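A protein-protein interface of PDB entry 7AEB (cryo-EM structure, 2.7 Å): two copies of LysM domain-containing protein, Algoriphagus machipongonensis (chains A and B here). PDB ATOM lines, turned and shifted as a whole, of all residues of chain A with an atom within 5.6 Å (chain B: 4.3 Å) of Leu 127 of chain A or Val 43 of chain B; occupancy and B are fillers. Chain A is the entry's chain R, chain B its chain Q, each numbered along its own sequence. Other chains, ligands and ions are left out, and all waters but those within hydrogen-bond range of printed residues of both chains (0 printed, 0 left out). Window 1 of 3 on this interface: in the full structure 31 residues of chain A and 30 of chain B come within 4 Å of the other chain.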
ATOM      1  N   VAL A 101     -20.173 -21.568  24.903  1.00  0.00           N
ATOM      2  CA  VAL A 101     -19.545 -22.221  23.761  1.00  0.00           C
ATOM      3  C   VAL A 101     -18.042 -21.959  23.634  1.00  0.00           C
ATOM      4  O   VAL A 101     -17.355 -22.724  22.947  1.00  0.00           O
ATOM      5  CB  VAL A 101     -20.275 -21.852  22.449  1.00  0.00           C
ATOM      6  CG1 VAL A 101     -21.771 -22.107  22.577  1.00  0.00           C
ATOM      7  CG2 VAL A 101     -19.998 -20.411  22.036  1.00  0.00           C
ATOM      8  N   TYR A 102     -17.499 -20.938  24.287  1.00  0.00           N
ATOM      9  CA  TYR A 102     -16.116 -20.542  24.027  1.00  0.00           C
ATOM     10  C   TYR A 102     -15.181 -20.667  25.223  1.00  0.00           C
ATOM     11  O   TYR A 102     -14.037 -21.089  25.052  1.00  0.00           O
ATOM     12  CB  TYR A 102     -16.081 -19.096  23.502  1.00  0.00           C
ATOM     13  CG  TYR A 102     -14.692 -18.571  23.230  1.00  0.00           C
ATOM     14  CD1 TYR A 102     -13.963 -19.011  22.134  1.00  0.00           C
ATOM     15  CD2 TYR A 102     -14.112 -17.630  24.068  1.00  0.00           C
ATOM     16  CE1 TYR A 102     -12.692 -18.535  21.891  1.00  0.00           C
ATOM     17  CE2 TYR A 102     -12.853 -17.153  23.832  1.00  0.00           C
ATOM     18  CZ  TYR A 102     -12.148 -17.605  22.748  1.00  0.00           C
ATOM     19  OH  TYR A 102     -10.893 -17.112  22.521  1.00  0.00           O
ATOM     20  N   PRO A 111     -12.317 -26.187  26.886  1.00  0.00           N
ATOM     21  CA  PRO A 111     -13.702 -25.729  26.687  1.00  0.00           C
ATOM     22  C   PRO A 111     -14.701 -26.882  26.741  1.00  0.00           C
ATOM     23  O   PRO A 111     -14.336 -28.056  26.796  1.00  0.00           O
ATOM     24  CB  PRO A 111     -13.667 -25.084  25.300  1.00  0.00           C
ATOM     25  CG  PRO A 111     -12.244 -24.752  25.062  1.00  0.00           C
ATOM     26  CD  PRO A 111     -11.455 -25.801  25.751  1.00  0.00           C
ATOM     27  N   LEU A 114     -20.534 -29.748  23.622  1.00  0.00           N
ATOM     28  CA  LEU A 114     -21.756 -29.078  23.205  1.00  0.00           C
ATOM     29  C   LEU A 114     -22.735 -30.066  22.594  1.00  0.00           C
ATOM     30  O   LEU A 114     -22.339 -30.951  21.840  1.00  0.00           O
ATOM     31  CB  LEU A 114     -21.468 -27.976  22.187  1.00  0.00           C
ATOM     32  CG  LEU A 114     -20.424 -26.922  22.533  1.00  0.00           C
ATOM     33  CD1 LEU A 114     -20.161 -26.056  21.321  1.00  0.00           C
ATOM     34  CD2 LEU A 114     -20.866 -26.091  23.721  1.00  0.00           C
ATOM     35  N   GLY A 125     -20.342 -31.913  19.576  1.00  0.00           N
ATOM     36  CA  GLY A 125     -18.983 -31.611  19.186  1.00  0.00           C
ATOM     37  C   GLY A 125     -18.348 -30.432  19.881  1.00  0.00           C
ATOM     38  O   GLY A 125     -18.576 -30.190  21.067  1.00  0.00           O
ATOM     39  N   TYR A 126     -17.527 -29.710  19.118  1.00  0.00           N
ATOM     40  CA  TYR A 126     -16.645 -28.652  19.590  1.00  0.00           C
ATOM     41  C   TYR A 126     -16.755 -27.428  18.700  1.00  0.00           C
ATOM     42  O   TYR A 126     -16.925 -27.544  17.487  1.00  0.00           O
ATOM     43  CB  TYR A 126     -15.183 -29.086  19.565  1.00  0.00           C
ATOM     44  CG  TYR A 126     -14.693 -29.844  20.756  1.00  0.00           C
ATOM     45  CD1 TYR A 126     -15.241 -29.646  22.010  1.00  0.00           C
ATOM     46  CD2 TYR A 126     -13.678 -30.775  20.618  1.00  0.00           C
ATOM     47  CE1 TYR A 126     -14.779 -30.346  23.099  1.00  0.00           C
ATOM     48  CE2 TYR A 126     -13.214 -31.485  21.694  1.00  0.00           C
ATOM     49  CZ  TYR A 126     -13.765 -31.266  22.928  1.00  0.00           C
ATOM     50  OH  TYR A 126     -13.294 -31.980  23.994  1.00  0.00           O
ATOM     51  N   LEU A 127     -16.588 -26.255  19.299  1.00  0.00           N
ATOM     52  CA  LEU A 127     -16.454 -25.026  18.530  1.00  0.00           C
ATOM     53  C   LEU A 127     -15.066 -24.933  17.903  1.00  0.00           C
ATOM     54  O   LEU A 127     -14.056 -25.221  18.546  1.00  0.00           O
ATOM     55  CB  LEU A 127     -16.703 -23.813  19.425  1.00  0.00           C
ATOM     56  CG  LEU A 127     -16.437 -22.417  18.857  1.00  0.00           C
ATOM     57  CD1 LEU A 127     -17.539 -22.007  17.924  1.00  0.00           C
ATOM     58  CD2 LEU A 127     -16.278 -21.406  19.953  1.00  0.00           C
ATOM     59  N   LYS A 128     -15.017 -24.527  16.639  1.00  0.00           N
ATOM     60  CA  LYS A 128     -13.750 -24.234  15.980  1.00  0.00           C
ATOM     61  C   LYS A 128     -13.538 -22.759  15.685  1.00  0.00           C
ATOM     62  O   LYS A 128     -12.428 -22.263  15.857  1.00  0.00           O
ATOM     63  CB  LYS A 128     -13.634 -25.017  14.673  1.00  0.00           C
ATOM     64  CG  LYS A 128     -13.795 -26.495  14.820  1.00  0.00           C
ATOM     65  CD  LYS A 128     -14.051 -27.130  13.479  1.00  0.00           C
ATOM     66  CE  LYS A 128     -12.759 -27.329  12.724  1.00  0.00           C
ATOM     67  NZ  LYS A 128     -12.956 -28.121  11.497  1.00  0.00           N
ATOM     68  N   GLU A 129     -14.571 -22.042  15.245  1.00  0.00           N
ATOM     69  CA  GLU A 129     -14.419 -20.694  14.716  1.00  0.00           C
ATOM     70  C   GLU A 129     -15.630 -19.843  15.055  1.00  0.00           C
ATOM     71  O   GLU A 129     -16.755 -20.339  15.110  1.00  0.00           O
ATOM     72  CB  GLU A 129     -14.243 -20.699  13.201  1.00  0.00           C
ATOM     73  CG  GLU A 129     -12.831 -20.892  12.755  1.00  0.00           C
ATOM     74  CD  GLU A 129     -12.747 -21.326  11.318  1.00  0.00           C
ATOM     75  OE1 GLU A 129     -13.428 -20.709  10.475  1.00  0.00           O
ATOM     76  OE2 GLU A 129     -12.009 -22.290  11.029  1.00  0.00           O
ATOM     77  N   MET A 130     -15.392 -18.549  15.242  1.00  0.00           N
ATOM     78  CA  MET A 130     -16.459 -17.605  15.539  1.00  0.00           C
ATOM     79  C   MET A 130     -16.040 -16.201  15.119  1.00  0.00           C
ATOM     80  O   MET A 130     -14.877 -15.824  15.260  1.00  0.00           O
ATOM     81  CB  MET A 130     -16.820 -17.646  17.027  1.00  0.00           C
ATOM     82  CG  MET A 130     -18.180 -17.074  17.336  1.00  0.00           C
ATOM     83  SD  MET A 130     -18.767 -17.485  18.975  1.00  0.00           S
ATOM     84  CE  MET A 130     -17.443 -16.870  20.002  1.00  0.00           C
ATOM     85  N   THR A 150     -20.558 -19.180  12.857  1.00  0.00           N
ATOM     86  CA  THR A 150     -20.092 -20.241  13.744  1.00  0.00           C
ATOM     87  C   THR A 150     -19.747 -21.486  12.925  1.00  0.00           C
ATOM     88  O   THR A 150     -20.361 -21.753  11.891  1.00  0.00           O
ATOM     89  CB  THR A 150     -21.170 -20.548  14.814  1.00  0.00           C
ATOM     90  OG1 THR A 150     -21.610 -19.327  15.417  1.00  0.00           O
ATOM     91  CG2 THR A 150     -20.635 -21.391  15.925  1.00  0.00           C
ATOM     92  N   LYS A 151     -18.752 -22.246  13.386  1.00  0.00           N
ATOM     93  CA  LYS A 151     -18.371 -23.517  12.780  1.00  0.00           C
ATOM     94  C   LYS A 151     -18.125 -24.557  13.867  1.00  0.00           C
ATOM     95  O   LYS A 151     -17.342 -24.316  14.787  1.00  0.00           O
ATOM     96  CB  LYS A 151     -17.122 -23.346  11.918  1.00  0.00           C
ATOM     97  CG  LYS A 151     -16.754 -24.567  11.122  1.00  0.00           C
ATOM     98  CD  LYS A 151     -15.527 -24.318  10.284  1.00  0.00           C
ATOM     99  CE  LYS A 151     -15.038 -25.604   9.651  1.00  0.00           C
ATOM    100  NZ  LYS A 151     -13.771 -25.431   8.904  1.00  0.00           N
ATOM    101  N   ILE A 152     -18.788 -25.712  13.759  1.00  0.00           N
ATOM    102  CA  ILE A 152     -18.763 -26.755  14.786  1.00  0.00           C
ATOM    103  C   ILE A 152     -18.174 -28.034  14.198  1.00  0.00           C
ATOM    104  O   ILE A 152     -18.563 -28.458  13.108  1.00  0.00           O
ATOM    105  CB  ILE A 152     -20.170 -27.036  15.356  1.00  0.00           C
ATOM    106  CG1 ILE A 152     -20.919 -25.741  15.669  1.00  0.00           C
ATOM    107  CG2 ILE A 152     -20.091 -27.894  16.607  1.00  0.00           C
ATOM    108  CD1 ILE A 152     -20.406 -24.998  16.873  1.00  0.00           C
ATOM    109  N   GLY A 153     -17.255 -28.659  14.937  1.00  0.00           N
ATOM    110  CA  GLY A 153     -16.748 -29.973  14.592  1.00  0.00           C
ATOM    111  C   GLY A 153     -17.515 -31.089  15.279  1.00  0.00           C
ATOM    112  O   GLY A 153     -18.375 -30.845  16.109  1.00  0.00           O
ATOM    113  N   ARG B  42     -10.640 -18.188  17.559  1.00  0.00           N
ATOM    114  CA  ARG B  42     -10.141 -19.417  16.944  1.00  0.00           C
ATOM    115  C   ARG B  42      -9.730 -20.425  18.010  1.00  0.00           C
ATOM    116  O   ARG B  42      -9.028 -20.076  18.960  1.00  0.00           O
ATOM    117  CB  ARG B  42      -8.939 -19.144  16.029  1.00  0.00           C
ATOM    118  CG  ARG B  42      -9.206 -18.261  14.821  1.00  0.00           C
ATOM    119  CD  ARG B  42     -10.237 -18.885  13.917  1.00  0.00           C
ATOM    120  NE  ARG B  42     -10.511 -18.081  12.732  1.00  0.00           N
ATOM    121  CZ  ARG B  42     -11.541 -17.254  12.604  1.00  0.00           C
ATOM    122  NH1 ARG B  42     -12.401 -17.100  13.592  1.00  0.00           N
ATOM    123  NH2 ARG B  42     -11.707 -16.575  11.485  1.00  0.00           N
ATOM    124  N   VAL B  43     -10.164 -21.674  17.851  1.00  0.00           N
ATOM    125  CA  VAL B  43      -9.773 -22.782  18.726  1.00  0.00           C
ATOM    126  C   VAL B  43      -9.197 -23.888  17.852  1.00  0.00           C
ATOM    127  O   VAL B  43      -9.787 -24.241  16.827  1.00  0.00           O
ATOM    128  CB  VAL B  43     -10.950 -23.319  19.572  1.00  0.00           C
ATOM    129  CG1 VAL B  43     -10.463 -24.346  20.576  1.00  0.00           C
ATOM    130  CG2 VAL B  43     -11.653 -22.209  20.311  1.00  0.00           C
ATOM    131  N   GLU B  44      -8.038 -24.413  18.246  1.00  0.00           N
ATOM    132  CA  GLU B  44      -7.325 -25.429  17.475  1.00  0.00           C
ATOM    133  C   GLU B  44      -7.357 -26.814  18.110  1.00  0.00           C
ATOM    134  O   GLU B  44      -7.189 -26.966  19.322  1.00  0.00           O
ATOM    135  CB  GLU B  44      -5.877 -24.995  17.236  1.00  0.00           C
ATOM    136  CG  GLU B  44      -5.044 -26.002  16.460  1.00  0.00           C
ATOM    137  CD  GLU B  44      -3.619 -25.543  16.247  1.00  0.00           C
ATOM    138  OE1 GLU B  44      -3.255 -24.472  16.771  1.00  0.00           O
ATOM    139  OE2 GLU B  44      -2.847 -26.274  15.591  1.00  0.00           O
ATOM    140  N   GLN B  45      -7.573 -27.828  17.275  1.00  0.00           N
ATOM    141  CA  GLN B  45      -7.653 -29.210  17.723  1.00  0.00           C
ATOM    142  C   GLN B  45      -6.653 -30.080  16.979  1.00  0.00           C
ATOM    143  O   GLN B  45      -6.165 -29.721  15.907  1.00  0.00           O
ATOM    144  CB  GLN B  45      -9.056 -29.794  17.530  1.00  0.00           C
ATOM    145  CG  GLN B  45     -10.072 -29.327  18.538  1.00  0.00           C
ATOM    146  CD  GLN B  45     -10.927 -28.219  17.998  1.00  0.00           C
ATOM    147  OE1 GLN B  45     -10.935 -27.962  16.803  1.00  0.00           O
ATOM    148  NE2 GLN B  45     -11.643 -27.544  18.877  1.00  0.00           N
ATOM    149  N   LYS B  62      -5.285 -25.804  21.816  1.00  0.00           N
ATOM    150  CA  LYS B  62      -4.926 -24.433  22.164  1.00  0.00           C
ATOM    151  C   LYS B  62      -6.072 -23.482  21.862  1.00  0.00           C
ATOM    152  O   LYS B  62      -6.912 -23.742  21.006  1.00  0.00           O
ATOM    153  CB  LYS B  62      -3.689 -23.967  21.391  1.00  0.00           C
ATOM    154  CG  LYS B  62      -2.409 -24.022  22.152  1.00  0.00           C
ATOM    155  CD  LYS B  62      -1.285 -23.417  21.361  1.00  0.00           C
ATOM    156  CE  LYS B  62      -1.107 -24.079  20.032  1.00  0.00           C
ATOM    157  NZ  LYS B  62       0.273 -23.904  19.540  1.00  0.00           N
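No position is printed for both chains.
Tyr 126 of chain A touches Gln 45 of chain B (CB to NE2, 3.9 Å). Leu 127 of chain A touches Val 43 of chain B. Arg 42 of chain B touches Lys 128 of chain A. OE1 of Gln 45 of chain B touches CG of Lys 128 of chain A (3.8 Å). CG of Glu 129 of chain A touches CD of Arg 42 of chain B (3.5 Å).
The backbone NH (N) of Gly 153 of chain A lies within hydrogen-bond range of the backbone carbonyl oxygen (O) of Tyr 126 of chain A (2.8 Å). The backbone NH (N) of Lys 128 of chain A is in hydrogen-bond range of the backbone carbonyl oxygen (O) of Lys 151 of chain A, 3.0 Å away. N of Lys 151 of chain A is in hydrogen-bond range of O of Glu 129 of chain A (3.3 Å).
Of the 14 printed residues of chain A, 5 touch a printed residue of chain B. Among the printed residues, 8 pairs touch across the chains. Among the printed residues, no Asp or Glu carboxylate lies within 4 Å of a Lys or Arg side-chain nitrogen of the other chain.
The guanidinium group (NH1) of Arg 42 of chain B is in hydrogen-bond range of the backbone carbonyl oxygen (O) of Met 130 of chain A, at 3.2 Å. O of Lys 128 of chain A sits at hydrogen-bond distance from N of Val 43 of chain B, 3.1 Å away. The backbone carbonyl oxygen (O) of Leu 127 of chain A is in hydrogen-bond range of the side-chain amide nitrogen (NE2) of Gln 45 of chain B (3.4 Å).
Of the printed residues of chain B, Tyr 126 of chain A touches Gln 45 (3.9 Å). Of chain B, only Val 43 and Gln 45 come within 4 Å of Leu 127 of chain A. Of the printed residues of chain B, Glu 129 of chain A touches Arg 42 (3.5 Å). Of the printed residues of chain B, Met 130 of chain A touches Arg 42. Of the printed residues of chain A, Arg 42 of chain B touches Lys 128, Glu 129 and Met 130. Of the printed residues of chain A, Val 43 of chain B touches Leu 127 (3.8 Å) and Lys 128 (3.1 Å). Of the printed residues of chain A, Gln 45 of chain B touches Tyr 126 (3.9 Å), Leu 127 (3.4 Å) and Lys 128 (3.8 Å). The nearest printed residue of chain B that does not touch Leu 127 of chain A is Glu 44 of chain B (6.1 Å).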
